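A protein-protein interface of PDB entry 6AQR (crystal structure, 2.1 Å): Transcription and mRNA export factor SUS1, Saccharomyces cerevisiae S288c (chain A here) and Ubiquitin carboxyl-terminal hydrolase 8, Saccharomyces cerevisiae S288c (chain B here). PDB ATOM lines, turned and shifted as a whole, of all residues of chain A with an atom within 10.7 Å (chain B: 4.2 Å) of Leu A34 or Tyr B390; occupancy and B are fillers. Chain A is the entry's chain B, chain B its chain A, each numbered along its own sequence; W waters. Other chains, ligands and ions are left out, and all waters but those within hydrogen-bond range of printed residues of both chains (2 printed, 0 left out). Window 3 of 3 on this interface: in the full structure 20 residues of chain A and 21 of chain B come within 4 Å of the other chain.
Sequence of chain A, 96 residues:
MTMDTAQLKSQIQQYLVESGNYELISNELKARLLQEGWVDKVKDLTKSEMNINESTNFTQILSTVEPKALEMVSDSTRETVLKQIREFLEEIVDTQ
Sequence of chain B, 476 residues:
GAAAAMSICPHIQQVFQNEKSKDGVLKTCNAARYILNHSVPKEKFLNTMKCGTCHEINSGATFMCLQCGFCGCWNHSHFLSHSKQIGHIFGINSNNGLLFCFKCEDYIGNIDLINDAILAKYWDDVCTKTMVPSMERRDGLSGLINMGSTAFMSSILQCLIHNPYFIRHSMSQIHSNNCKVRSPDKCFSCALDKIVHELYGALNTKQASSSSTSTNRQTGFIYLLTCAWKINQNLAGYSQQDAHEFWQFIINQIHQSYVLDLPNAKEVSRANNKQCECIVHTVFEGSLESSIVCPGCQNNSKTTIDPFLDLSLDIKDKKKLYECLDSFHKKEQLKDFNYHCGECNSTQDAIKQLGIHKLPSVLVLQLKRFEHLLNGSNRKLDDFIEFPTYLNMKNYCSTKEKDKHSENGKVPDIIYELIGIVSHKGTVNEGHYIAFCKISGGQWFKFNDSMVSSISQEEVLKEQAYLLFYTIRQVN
The side-chain carboxylate of Glu B417 lies within salt-bridge range of the side-chain amino group of Lys B438 (2.7 Å).
The side-chain hydroxyl (OH) of Tyr B390 lies within hydrogen-bond range of the side-chain amino group (NZ) of Lys B438, 3.5 Å away.
The backbone NH (N) of Arg B473 is in hydrogen-bond range of the backbone carbonyl oxygen (O) of Ile B415 (2.8 Å).
The side-chain carboxylate (OE2) of Glu B417 is in salt-bridge range of the guanidinium group (NH1) of Arg B473 (2.9 Å).
The backbone carbonyl oxygen (O) of Gln B474 lies within hydrogen-bond range of the backbone NH (N) of Ile B415 (2.8 Å).
NE2 of Gln A35 lies within hydrogen-bond range of O of Ala A31, at 3.2 Å.
Of the 11 printed residues of chain B, 5 touch a printed residue of chain A.
Hydrophobic or aromatic side chains of chain B within 4 Å of the printed part of chain A: Tyr B390 and Ile B415.
Hydrophobic or aromatic side chains of chain A that line the printed part of chain B: Ala A31 and Leu A34.
Among the printed residues, Asp or Glu carboxylates within 4 Å of a Lys or Arg side-chain nitrogen of the other chain: Asp A40 with Lys B438 (2.8 Å).
Water W1 lies within hydrogen-bond range of OG1 of Thr B389 (2.7 Å), N of Tyr B390 (3.0 Å) and O of Gln A35 (3.1 Å).
Water W2 bridges NZ of Lys A30 and OE1 of Gln B474.
O of Asn A27 sits at hydrogen-bond distance from NE2 of Gln B474, 2.9 Å away.
NZ of Lys B438 is in salt-bridge range of OD2 of Asp A40, at 2.8 Å.
The side-chain carboxylate (OD1) of Asp A40 sits at hydrogen-bond distance from the side-chain hydroxyl (OH) of Tyr B390, at 2.6 Å.
Among the printed residues, merely in contact across the chains: Lys A30 with Gln B474 (3.3 Å), Ala A31 with Gln B474 (3.6 Å), Leu A34 with Tyr B390 (3.3 Å), Leu A34 with Arg B473 (3.95 Å) and Gln A35 with Ile B415 (3.6 Å).
Leu A34 touches just these residues of chain B: Tyr B390 (3.3 Å) and Arg B473 (3.95 Å).
Of the printed residues of chain B, Gln A35 touches Ile B415.
Gly A37 touches none of the printed residues of chain B.
Lys A41 touches none of the printed residues of chain B.
Pro B388 touches none of the printed residues of chain A.
No residue of chain A comes within 4 Å of Thr B389.
Of chain A, only Leu A34 and Asp A40 come within 4 Å of Tyr B390.
No residue of chain A comes within 4 Å of Leu B391.
No residue of chain A comes within 4 Å of Glu B417.
Printed residues of chain A within 4 Å of Gln B474: Asn A27, Lys A30 and Ala A31.
The nearest residue of chain A that does not touch Tyr B390 is Gln A35 (4.1 Å).
The nearest printed residue of chain A that does not touch Arg B473 is Lys A30 (4.3 Å).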
ATOM      1  N   SER A  26      -7.269 -35.841 -33.806  1.00  0.00           N
ATOM      2  CA  SER A  26      -8.213 -34.827 -34.198  1.00  0.00           C
ATOM      3  C   SER A  26      -9.393 -34.721 -33.222  1.00  0.00           C
ATOM      4  O   SER A  26      -9.687 -33.629 -32.713  1.00  0.00           O
ATOM      5  CB  SER A  26      -8.648 -35.098 -35.626  1.00  0.00           C
ATOM      6  OG  SER A  26      -9.491 -34.046 -36.045  1.00  0.00           O
ATOM      7  N   ASN A  27      -9.958 -35.840 -32.810  1.00  0.00           N
ATOM      8  CA  ASN A  27     -10.993 -35.795 -31.734  1.00  0.00           C
ATOM      9  C   ASN A  27     -10.609 -35.296 -30.372  1.00  0.00           C
ATOM     10  O   ASN A  27     -11.346 -34.577 -29.721  1.00  0.00           O
ATOM     11  CB  ASN A  27     -11.678 -37.144 -31.596  1.00  0.00           C
ATOM     12  CG  ASN A  27     -12.411 -37.508 -32.841  1.00  0.00           C
ATOM     13  OD1 ASN A  27     -12.770 -36.639 -33.681  1.00  0.00           O
ATOM     14  ND2 ASN A  27     -12.601 -38.782 -33.014  1.00  0.00           N
ATOM     15  N   GLU A  28      -9.442 -35.697 -29.936  1.00  0.00           N
ATOM     16  CA  GLU A  28      -8.906 -35.301 -28.664  1.00  0.00           C
ATOM     17  C   GLU A  28      -8.613 -33.791 -28.649  1.00  0.00           C
ATOM     18  O   GLU A  28      -8.962 -33.089 -27.697  1.00  0.00           O
ATOM     19  CB  GLU A  28      -7.627 -36.083 -28.472  1.00  0.00           C
ATOM     20  CG  GLU A  28      -6.690 -35.581 -27.372  1.00  0.00           C
ATOM     21  CD  GLU A  28      -7.190 -35.887 -25.964  1.00  0.00           C
ATOM     22  OE1 GLU A  28      -8.287 -36.493 -25.780  1.00  0.00           O
ATOM     23  OE2 GLU A  28      -6.478 -35.515 -25.016  1.00  0.00           O
ATOM     24  N   LEU A  29      -7.922 -33.315 -29.686  1.00  0.00           N
ATOM     25  CA  LEU A  29      -7.741 -31.843 -29.886  1.00  0.00           C
ATOM     26  C   LEU A  29      -9.072 -31.106 -29.801  1.00  0.00           C
ATOM     27  O   LEU A  29      -9.238 -30.197 -28.953  1.00  0.00           O
ATOM     28  CB  LEU A  29      -6.968 -31.542 -31.218  1.00  0.00           C
ATOM     29  CG  LEU A  29      -6.769 -30.076 -31.520  1.00  0.00           C
ATOM     30  CD1 LEU A  29      -5.950 -29.423 -30.420  1.00  0.00           C
ATOM     31  CD2 LEU A  29      -6.107 -29.873 -32.875  1.00  0.00           C
ATOM     32  N   LYS A  30     -10.040 -31.545 -30.609  1.00  0.00           N
ATOM     33  CA  LYS A  30     -11.393 -30.929 -30.575  1.00  0.00           C
ATOM     34  C   LYS A  30     -12.066 -30.996 -29.209  1.00  0.00           C
ATOM     35  O   LYS A  30     -12.557 -30.000 -28.701  1.00  0.00           O
ATOM     36  CB  LYS A  30     -12.307 -31.551 -31.620  1.00  0.00           C
ATOM     37  CG  LYS A  30     -13.641 -30.815 -31.789  1.00  0.00           C
ATOM     38  CD  LYS A  30     -13.447 -29.339 -32.123  1.00  0.00           C
ATOM     39  CE  LYS A  30     -14.775 -28.542 -32.176  1.00  0.00           C
ATOM     40  NZ  LYS A  30     -15.735 -29.222 -33.121  1.00  0.00           N
ATOM     41  N   ALA A  31     -12.047 -32.155 -28.573  1.00  0.00           N
ATOM     42  CA  ALA A  31     -12.593 -32.223 -27.240  1.00  0.00           C
ATOM     43  C   ALA A  31     -12.004 -31.220 -26.224  1.00  0.00           C
ATOM     44  O   ALA A  31     -12.736 -30.605 -25.453  1.00  0.00           O
ATOM     45  CB  ALA A  31     -12.522 -33.648 -26.711  1.00  0.00           C
ATOM     46  N   ARG A  32     -10.698 -31.031 -26.258  1.00  0.00           N
ATOM     47  CA  ARG A  32     -10.031 -30.223 -25.266  1.00  0.00           C
ATOM     48  C   ARG A  32     -10.253 -28.747 -25.547  1.00  0.00           C
ATOM     49  O   ARG A  32     -10.379 -27.961 -24.644  1.00  0.00           O
ATOM     50  CB  ARG A  32      -8.545 -30.511 -25.397  1.00  0.00           C
ATOM     51  CG  ARG A  32      -8.032 -31.318 -24.223  1.00  0.00           C
ATOM     52  CD  ARG A  32      -6.602 -31.755 -24.470  1.00  0.00           C
ATOM     53  NE  ARG A  32      -6.539 -33.170 -24.112  1.00  0.00           N
ATOM     54  CZ  ARG A  32      -6.358 -33.646 -22.877  1.00  0.00           C
ATOM     55  NH1 ARG A  32      -6.142 -32.844 -21.838  1.00  0.00           N
ATOM     56  NH2 ARG A  32      -6.371 -34.954 -22.685  1.00  0.00           N
ATOM     57  N   LEU A  33     -10.283 -28.378 -26.816  1.00  0.00           N
ATOM     58  CA  LEU A  33     -10.529 -26.974 -27.214  1.00  0.00           C
ATOM     59  C   LEU A  33     -11.932 -26.524 -26.814  1.00  0.00           C
ATOM     60  O   LEU A  33     -12.145 -25.405 -26.314  1.00  0.00           O
ATOM     61  CB  LEU A  33     -10.319 -26.833 -28.722  1.00  0.00           C
ATOM     62  CG  LEU A  33      -8.838 -26.911 -29.131  1.00  0.00           C
ATOM     63  CD1 LEU A  33      -8.635 -26.859 -30.662  1.00  0.00           C
ATOM     64  CD2 LEU A  33      -7.958 -25.862 -28.434  1.00  0.00           C
ATOM     65  N   LEU A  34     -12.882 -27.423 -27.045  1.00  0.00           N
ATOM     66  CA  LEU A  34     -14.263 -27.208 -26.715  1.00  0.00           C
ATOM     67  C   LEU A  34     -14.341 -26.976 -25.210  1.00  0.00           C
ATOM     68  O   LEU A  34     -14.811 -25.910 -24.772  1.00  0.00           O
ATOM     69  CB  LEU A  34     -15.016 -28.431 -27.117  1.00  0.00           C
ATOM     70  CG  LEU A  34     -16.425 -28.285 -27.629  1.00  0.00           C
ATOM     71  CD1 LEU A  34     -16.740 -27.136 -28.608  1.00  0.00           C
ATOM     72  CD2 LEU A  34     -16.646 -29.635 -28.224  1.00  0.00           C
ATOM     73  N   GLN A  35     -13.759 -27.893 -24.430  1.00  0.00           N
ATOM     74  CA  GLN A  35     -13.882 -27.817 -22.979  1.00  0.00           C
ATOM     75  C   GLN A  35     -13.153 -26.634 -22.347  1.00  0.00           C
ATOM     76  O   GLN A  35     -13.591 -26.139 -21.357  1.00  0.00           O
ATOM     77  CB  GLN A  35     -13.395 -29.124 -22.288  1.00  0.00           C
ATOM     78  CG  GLN A  35     -14.434 -30.222 -22.332  1.00  0.00           C
ATOM     79  CD  GLN A  35     -13.930 -31.555 -21.883  1.00  0.00           C
ATOM     80  OE1 GLN A  35     -14.293 -32.022 -20.825  1.00  0.00           O
ATOM     81  NE2 GLN A  35     -13.090 -32.169 -22.680  1.00  0.00           N
ATOM     82  N   GLU A  36     -12.011 -26.222 -22.876  1.00  0.00           N
ATOM     83  CA  GLU A  36     -11.336 -25.069 -22.314  1.00  0.00           C
ATOM     84  C   GLU A  36     -11.986 -23.713 -22.728  1.00  0.00           C
ATOM     85  O   GLU A  36     -11.524 -22.671 -22.296  1.00  0.00           O
ATOM     86  CB  GLU A  36      -9.859 -25.117 -22.656  1.00  0.00           C
ATOM     87  CG  GLU A  36      -9.485 -24.603 -24.034  1.00  0.00           C
ATOM     88  CD  GLU A  36      -8.004 -24.834 -24.370  1.00  0.00           C
ATOM     89  OE1 GLU A  36      -7.418 -25.845 -23.926  1.00  0.00           O
ATOM     90  OE2 GLU A  36      -7.410 -24.028 -25.117  1.00  0.00           O
ATOM     91  N   GLY A  37     -13.023 -23.730 -23.579  1.00  0.00           N
ATOM     92  CA  GLY A  37     -13.668 -22.493 -24.016  1.00  0.00           C
ATOM     93  C   GLY A  37     -13.116 -21.864 -25.278  1.00  0.00           C
ATOM     94  O   GLY A  37     -13.516 -20.762 -25.638  1.00  0.00           O
ATOM     95  N   TRP A  38     -12.200 -22.519 -25.954  1.00  0.00           N
ATOM     96  CA  TRP A  38     -11.509 -21.862 -27.049  1.00  0.00           C
ATOM     97  C   TRP A  38     -12.427 -21.666 -28.267  1.00  0.00           C
ATOM     98  O   TRP A  38     -12.301 -20.643 -28.973  1.00  0.00           O
ATOM     99  CB  TRP A  38     -10.341 -22.730 -27.439  1.00  0.00           C
ATOM    100  CG  TRP A  38      -9.494 -22.237 -28.571  1.00  0.00           C
ATOM    101  CD1 TRP A  38      -8.434 -21.388 -28.487  1.00  0.00           C
ATOM    102  CD2 TRP A  38      -9.604 -22.632 -29.939  1.00  0.00           C
ATOM    103  NE1 TRP A  38      -7.849 -21.243 -29.739  1.00  0.00           N
ATOM    104  CE2 TRP A  38      -8.563 -21.988 -30.647  1.00  0.00           C
ATOM    105  CE3 TRP A  38     -10.501 -23.470 -30.648  1.00  0.00           C
ATOM    106  CZ2 TRP A  38      -8.372 -22.169 -32.028  1.00  0.00           C
ATOM    107  CZ3 TRP A  38     -10.356 -23.612 -31.997  1.00  0.00           C
ATOM    108  CH2 TRP A  38      -9.285 -22.985 -32.689  1.00  0.00           C
ATOM    109  N   VAL A  39     -13.338 -22.629 -28.523  1.00  0.00           N
ATOM    110  CA  VAL A  39     -14.219 -22.506 -29.715  1.00  0.00           C
ATOM    111  C   VAL A  39     -15.085 -21.256 -29.548  1.00  0.00           C
ATOM    112  O   VAL A  39     -15.172 -20.453 -30.483  1.00  0.00           O
ATOM    113  CB  VAL A  39     -15.058 -23.779 -30.060  1.00  0.00           C
ATOM    114  CG1 VAL A  39     -16.028 -23.525 -31.252  1.00  0.00           C
ATOM    115  CG2 VAL A  39     -14.141 -24.969 -30.385  1.00  0.00           C
ATOM    116  N   ASP A  40     -15.689 -21.082 -28.357  1.00  0.00           N
ATOM    117  CA  ASP A  40     -16.513 -19.917 -28.039  1.00  0.00           C
ATOM    118  C   ASP A  40     -15.701 -18.632 -28.119  1.00  0.00           C
ATOM    119  O   ASP A  40     -16.226 -17.613 -28.581  1.00  0.00           O
ATOM    120  CB  ASP A  40     -17.223 -20.020 -26.671  1.00  0.00           C
ATOM    121  CG  ASP A  40     -18.253 -21.200 -26.618  1.00  0.00           C
ATOM    122  OD1 ASP A  40     -17.829 -22.376 -26.695  1.00  0.00           O
ATOM    123  OD2 ASP A  40     -19.485 -20.952 -26.550  1.00  0.00           O
ATOM    124  N   LYS A  41     -14.441 -18.680 -27.682  1.00  0.00           N
ATOM    125  CA  LYS A  41     -13.546 -17.512 -27.747  1.00  0.00           C
ATOM    126  C   LYS A  41     -13.239 -17.133 -29.209  1.00  0.00           C
ATOM    127  O   LYS A  41     -13.159 -15.938 -29.531  1.00  0.00           O
ATOM    128  CB  LYS A  41     -12.248 -17.747 -27.003  1.00  0.00           C
ATOM    129  CG  LYS A  41     -12.373 -17.572 -25.482  1.00  0.00           C
ATOM    130  CD  LYS A  41     -11.047 -17.939 -24.776  1.00  0.00           C
ATOM    131  CE  LYS A  41     -11.184 -18.858 -23.545  1.00  0.00           C
ATOM    132  NZ  LYS A  41     -12.085 -18.267 -22.486  1.00  0.00           N
ATOM    133  N   VAL A  42     -13.044 -18.134 -30.084  1.00  0.00           N
ATOM    134  CA  VAL A  42     -12.799 -17.837 -31.508  1.00  0.00           C
ATOM    135  C   VAL A  42     -14.054 -17.191 -32.171  1.00  0.00           C
ATOM    136  O   VAL A  42     -13.928 -16.237 -32.927  1.00  0.00           O
ATOM    137  CB  VAL A  42     -12.286 -19.088 -32.255  1.00  0.00           C
ATOM    138  CG1 VAL A  42     -12.148 -18.850 -33.750  1.00  0.00           C
ATOM    139  CG2 VAL A  42     -10.933 -19.510 -31.675  1.00  0.00           C
ATOM    140  N   LYS A  43     -15.250 -17.661 -31.817  1.00  0.00           N
ATOM    141  CA  LYS A  43     -16.488 -17.088 -32.265  1.00  0.00           C
ATOM    142  C   LYS A  43     -16.633 -15.644 -31.825  1.00  0.00           C
ATOM    143  O   LYS A  43     -16.998 -14.821 -32.649  1.00  0.00           O
ATOM    144  CB  LYS A  43     -17.687 -17.892 -31.767  1.00  0.00           C
ATOM    145  CG  LYS A  43     -17.853 -19.225 -32.496  1.00  0.00           C
ATOM    146  CD  LYS A  43     -19.156 -19.885 -32.082  1.00  0.00           C
ATOM    147  CE  LYS A  43     -19.273 -21.326 -32.584  1.00  0.00           C
ATOM    148  NZ  LYS A  43     -20.745 -21.564 -32.538  1.00  0.00           N
ATOM    149  N   ASP A  44     -16.359 -15.351 -30.548  1.00  0.00           N
ATOM    150  CA  ASP A  44     -16.326 -13.973 -30.015  1.00  0.00           C
ATOM    151  C   ASP A  44     -15.290 -13.055 -30.685  1.00  0.00           C
ATOM    152  O   ASP A  44     -15.614 -11.927 -31.042  1.00  0.00           O
ATOM    153  CB  ASP A  44     -16.097 -13.977 -28.526  1.00  0.00           C
ATOM    154  CG  ASP A  44     -17.287 -14.544 -27.762  1.00  0.00           C
ATOM    155  OD1 ASP A  44     -18.266 -15.046 -28.390  1.00  0.00           O
ATOM    156  OD2 ASP A  44     -17.255 -14.464 -26.514  1.00  0.00           O
ATOM    157  N   MET A  72      -4.333 -18.183 -28.639  1.00  0.00           N
ATOM    158  CA  MET A  72      -5.274 -18.484 -27.570  1.00  0.00           C
ATOM    159  C   MET A  72      -5.317 -19.949 -27.107  1.00  0.00           C
ATOM    160  O   MET A  72      -5.939 -20.226 -26.055  1.00  0.00           O
ATOM    161  CB  MET A  72      -6.683 -18.040 -27.937  1.00  0.00           C
ATOM    162  CG  MET A  72      -6.869 -16.542 -28.035  1.00  0.00           C
ATOM    163  SD  MET A  72      -8.376 -16.198 -28.994  1.00  0.00           S
ATOM    164  CE  MET A  72      -9.694 -16.553 -27.886  1.00  0.00           C
ATOM    165  N   VAL A  73      -4.742 -20.871 -27.903  1.00  0.00           N
ATOM    166  CA  VAL A  73      -4.643 -22.268 -27.505  1.00  0.00           C
ATOM    167  C   VAL A  73      -3.839 -22.405 -26.177  1.00  0.00           C
ATOM    168  O   VAL A  73      -2.717 -21.992 -26.123  1.00  0.00           O
ATOM    169  CB  VAL A  73      -4.000 -23.134 -28.608  1.00  0.00           C
ATOM    170  CG1 VAL A  73      -3.906 -24.610 -28.150  1.00  0.00           C
ATOM    171  CG2 VAL A  73      -4.840 -23.058 -29.883  1.00  0.00           C
ATOM    172  N   SER A  74      -4.434 -22.987 -25.133  1.00  0.00           N
ATOM    173  CA  SER A  74      -3.759 -23.193 -23.837  1.00  0.00           C
ATOM    174  C   SER A  74      -2.535 -24.046 -24.053  1.00  0.00           C
ATOM    175  O   SER A  74      -2.464 -24.843 -25.019  1.00  0.00           O
ATOM    176  CB  SER A  74      -4.695 -23.866 -22.805  1.00  0.00           C
ATOM    177  OG  SER A  74      -4.939 -25.260 -23.074  1.00  0.00           O
ATOM    178  N   THR A  77      -3.297 -27.733 -23.560  1.00  0.00           N
ATOM    179  CA  THR A  77      -3.838 -28.471 -24.713  1.00  0.00           C
ATOM    180  C   THR A  77      -2.696 -28.719 -25.696  1.00  0.00           C
ATOM    181  O   THR A  77      -2.541 -29.816 -26.246  1.00  0.00           O
ATOM    182  CB  THR A  77      -5.001 -27.690 -25.409  1.00  0.00           C
ATOM    183  OG1 THR A  77      -6.168 -27.754 -24.613  1.00  0.00           O
ATOM    184  CG2 THR A  77      -5.368 -28.284 -26.761  1.00  0.00           C
ATOM    185  N   VAL A  81      -1.487 -32.503 -26.772  1.00  0.00           N
ATOM    186  CA  VAL A  81      -1.732 -33.015 -28.114  1.00  0.00           C
ATOM    187  C   VAL A  81      -0.425 -33.299 -28.804  1.00  0.00           C
ATOM    188  O   VAL A  81      -0.328 -34.280 -29.559  1.00  0.00           O
ATOM    189  CB  VAL A  81      -2.648 -32.110 -28.981  1.00  0.00           C
ATOM    190  CG1 VAL A  81      -2.831 -32.711 -30.376  1.00  0.00           C
ATOM    191  CG2 VAL A  81      -3.984 -32.003 -28.306  1.00  0.00           C
ATOM    192  N   TYR B 322     -19.606 -31.399 -11.045  1.00  0.00           N
ATOM    193  CA  TYR B 322     -18.997 -32.774 -11.193  1.00  0.00           C
ATOM    194  C   TYR B 322     -19.026 -33.492  -9.824  1.00  0.00           C
ATOM    195  O   TYR B 322     -19.137 -34.699  -9.762  1.00  0.00           O
ATOM    196  CB  TYR B 322     -17.558 -32.656 -11.647  1.00  0.00           C
ATOM    197  CG  TYR B 322     -17.416 -32.535 -13.145  1.00  0.00           C
ATOM    198  CD1 TYR B 322     -17.804 -33.609 -13.981  1.00  0.00           C
ATOM    199  CD2 TYR B 322     -16.843 -31.373 -13.746  1.00  0.00           C
ATOM    200  CE1 TYR B 322     -17.676 -33.512 -15.368  1.00  0.00           C
ATOM    201  CE2 TYR B 322     -16.701 -31.245 -15.143  1.00  0.00           C
ATOM    202  CZ  TYR B 322     -17.119 -32.302 -15.956  1.00  0.00           C
ATOM    203  OH  TYR B 322     -17.001 -32.257 -17.362  1.00  0.00           O
ATOM    204  N   PRO B 388     -20.040 -26.190 -15.634  1.00  0.00           N
ATOM    205  CA  PRO B 388     -19.169 -25.862 -16.741  1.00  0.00           C
ATOM    206  C   PRO B 388     -19.971 -25.615 -18.065  1.00  0.00           C
ATOM    207  O   PRO B 388     -21.111 -26.032 -18.196  1.00  0.00           O
ATOM    208  CB  PRO B 388     -18.355 -27.123 -16.911  1.00  0.00           C
ATOM    209  CG  PRO B 388     -19.408 -28.255 -16.624  1.00  0.00           C
ATOM    210  CD  PRO B 388     -20.151 -27.661 -15.422  1.00  0.00           C
ATOM    211  N   THR B 389     -19.324 -24.983 -19.064  1.00  0.00           N
ATOM    212  CA  THR B 389     -20.000 -24.612 -20.248  1.00  0.00           C
ATOM    213  C   THR B 389     -20.067 -25.873 -21.111  1.00  0.00           C
ATOM    214  O   THR B 389     -20.906 -25.945 -22.012  1.00  0.00           O
ATOM    215  CB  THR B 389     -19.212 -23.496 -20.997  1.00  0.00           C
ATOM    216  OG1 THR B 389     -17.823 -23.834 -20.950  1.00  0.00           O
ATOM    217  CG2 THR B 389     -19.435 -22.102 -20.332  1.00  0.00           C
ATOM    218  N   TYR B 390     -19.172 -26.814 -20.888  1.00  0.00           N
ATOM    219  CA  TYR B 390     -19.148 -28.115 -21.601  1.00  0.00           C
ATOM    220  C   TYR B 390     -18.971 -29.181 -20.542  1.00  0.00           C
ATOM    221  O   TYR B 390     -18.113 -29.017 -19.647  1.00  0.00           O
ATOM    222  CB  TYR B 390     -18.005 -28.168 -22.634  1.00  0.00           C
ATOM    223  CG  TYR B 390     -18.276 -27.197 -23.774  1.00  0.00           C
ATOM    224  CD1 TYR B 390     -17.892 -25.838 -23.676  1.00  0.00           C
ATOM    225  CD2 TYR B 390     -19.043 -27.590 -24.912  1.00  0.00           C
ATOM    226  CE1 TYR B 390     -18.224 -24.930 -24.697  1.00  0.00           C
ATOM    227  CE2 TYR B 390     -19.380 -26.682 -25.921  1.00  0.00           C
ATOM    228  CZ  TYR B 390     -18.957 -25.375 -25.807  1.00  0.00           C
ATOM    229  OH  TYR B 390     -19.290 -24.507 -26.859  1.00  0.00           O
ATOM    230  N   LEU B 391     -19.790 -30.230 -20.597  1.00  0.00           N
ATOM    231  CA  LEU B 391     -19.821 -31.258 -19.519  1.00  0.00           C
ATOM    232  C   LEU B 391     -19.441 -32.625 -20.084  1.00  0.00           C
ATOM    233  O   LEU B 391     -20.012 -33.032 -21.101  1.00  0.00           O
ATOM    234  CB  LEU B 391     -21.237 -31.280 -18.886  1.00  0.00           C
ATOM    235  CG  LEU B 391     -21.506 -32.390 -17.852  1.00  0.00           C
ATOM    236  CD1 LEU B 391     -20.742 -32.145 -16.524  1.00  0.00           C
ATOM    237  CD2 LEU B 391     -22.991 -32.299 -17.570  1.00  0.00           C
ATOM    238  N   ILE B 415     -19.233 -35.304 -24.541  1.00  0.00           N
ATOM    239  CA  ILE B 415     -19.253 -33.934 -24.128  1.00  0.00           C
ATOM    240  C   ILE B 415     -20.574 -33.317 -24.573  1.00  0.00           C
ATOM    241  O   ILE B 415     -20.950 -33.437 -25.780  1.00  0.00           O
ATOM    242  CB  ILE B 415     -18.120 -33.073 -24.830  1.00  0.00           C
ATOM    243  CG1 ILE B 415     -16.693 -33.678 -24.809  1.00  0.00           C
ATOM    244  CG2 ILE B 415     -18.196 -31.616 -24.358  1.00  0.00           C
ATOM    245  CD1 ILE B 415     -16.111 -33.972 -23.474  1.00  0.00           C
ATOM    246  N   TYR B 416     -21.245 -32.635 -23.618  1.00  0.00           N
ATOM    247  CA  TYR B 416     -22.476 -31.890 -23.852  1.00  0.00           C
ATOM    248  C   TYR B 416     -22.109 -30.399 -23.733  1.00  0.00           C
ATOM    249  O   TYR B 416     -21.220 -30.055 -22.958  1.00  0.00           O
ATOM    250  CB  TYR B 416     -23.468 -32.171 -22.726  1.00  0.00           C
ATOM    251  CG  TYR B 416     -24.108 -33.515 -22.775  1.00  0.00           C
ATOM    252  CD1 TYR B 416     -23.438 -34.677 -22.329  1.00  0.00           C
ATOM    253  CD2 TYR B 416     -25.381 -33.639 -23.332  1.00  0.00           C
ATOM    254  CE1 TYR B 416     -24.066 -35.913 -22.382  1.00  0.00           C
ATOM    255  CE2 TYR B 416     -26.026 -34.845 -23.361  1.00  0.00           C
ATOM    256  CZ  TYR B 416     -25.352 -35.982 -22.928  1.00  0.00           C
ATOM    257  OH  TYR B 416     -25.999 -37.175 -23.048  1.00  0.00           O
ATOM    258  N   GLU B 417     -22.855 -29.550 -24.414  1.00  0.00           N
ATOM    259  CA  GLU B 417     -22.704 -28.119 -24.313  1.00  0.00           C
ATOM    260  C   GLU B 417     -23.860 -27.597 -23.520  1.00  0.00           C
ATOM    261  O   GLU B 417     -24.991 -27.915 -23.864  1.00  0.00           O
ATOM    262  CB  GLU B 417     -22.794 -27.539 -25.742  1.00  0.00           C
ATOM    263  CG  GLU B 417     -22.883 -26.008 -25.846  1.00  0.00           C
ATOM    264  CD  GLU B 417     -22.878 -25.494 -27.346  1.00  0.00           C
ATOM    265  OE1 GLU B 417     -22.892 -24.269 -27.592  1.00  0.00           O
ATOM    266  OE2 GLU B 417     -22.936 -26.306 -28.312  1.00  0.00           O
ATOM    267  N   LYS B 438     -28.844 -20.068 -24.597  1.00  0.00           N
ATOM    268  CA  LYS B 438     -27.739 -19.811 -25.483  1.00  0.00           C
ATOM    269  C   LYS B 438     -28.212 -20.122 -26.892  1.00  0.00           C
ATOM    270  O   LYS B 438     -28.870 -21.126 -27.109  1.00  0.00           O
ATOM    271  CB  LYS B 438     -26.547 -20.725 -25.138  1.00  0.00           C
ATOM    272  CG  LYS B 438     -25.224 -20.385 -25.860  1.00  0.00           C
ATOM    273  CD  LYS B 438     -24.186 -21.475 -25.573  1.00  0.00           C
ATOM    274  CE  LYS B 438     -22.825 -21.254 -26.203  1.00  0.00           C
ATOM    275  NZ  LYS B 438     -21.863 -22.397 -25.935  1.00  0.00           N
ATOM    276  N   ARG B 473     -22.737 -32.956 -27.920  1.00  0.00           N
ATOM    277  CA  ARG B 473     -21.877 -32.253 -28.863  1.00  0.00           C
ATOM    278  C   ARG B 473     -20.880 -33.174 -29.467  1.00  0.00           C
ATOM    279  O   ARG B 473     -20.706 -33.188 -30.680  1.00  0.00           O
ATOM    280  CB  ARG B 473     -21.127 -31.164 -28.160  1.00  0.00           C
ATOM    281  CG  ARG B 473     -21.861 -29.892 -28.024  1.00  0.00           C
ATOM    282  CD  ARG B 473     -22.367 -29.340 -29.372  1.00  0.00           C
ATOM    283  NE  ARG B 473     -21.356 -29.226 -30.408  1.00  0.00           N
ATOM    284  CZ  ARG B 473     -20.501 -28.227 -30.559  1.00  0.00           C
ATOM    285  NH1 ARG B 473     -20.519 -27.155 -29.772  1.00  0.00           N
ATOM    286  NH2 ARG B 473     -19.642 -28.296 -31.569  1.00  0.00           N
ATOM    287  N   GLN B 474     -20.234 -33.995 -28.641  1.00  0.00           N
ATOM    288  CA  GLN B 474     -19.193 -34.820 -29.181  1.00  0.00           C
ATOM    289  C   GLN B 474     -19.148 -36.120 -28.487  1.00  0.00           C
ATOM    290  O   GLN B 474     -19.113 -36.148 -27.253  1.00  0.00           O
ATOM    291  CB  GLN B 474     -17.836 -34.060 -29.065  1.00  0.00           C
ATOM    292  CG  GLN B 474     -16.622 -34.945 -29.281  1.00  0.00           C
ATOM    293  CD  GLN B 474     -15.408 -34.159 -29.816  1.00  0.00           C
ATOM    294  OE1 GLN B 474     -15.520 -33.022 -30.280  1.00  0.00           O
ATOM    295  NE2 GLN B 474     -14.250 -34.783 -29.771  1.00  0.00           N
HETATM  296  O   HOH W   1     -16.399 -25.936 -20.006  1.00  0.00           O
HETATM  297  O   HOH W   2     -17.053 -31.156 -31.755  1.00  0.00           O
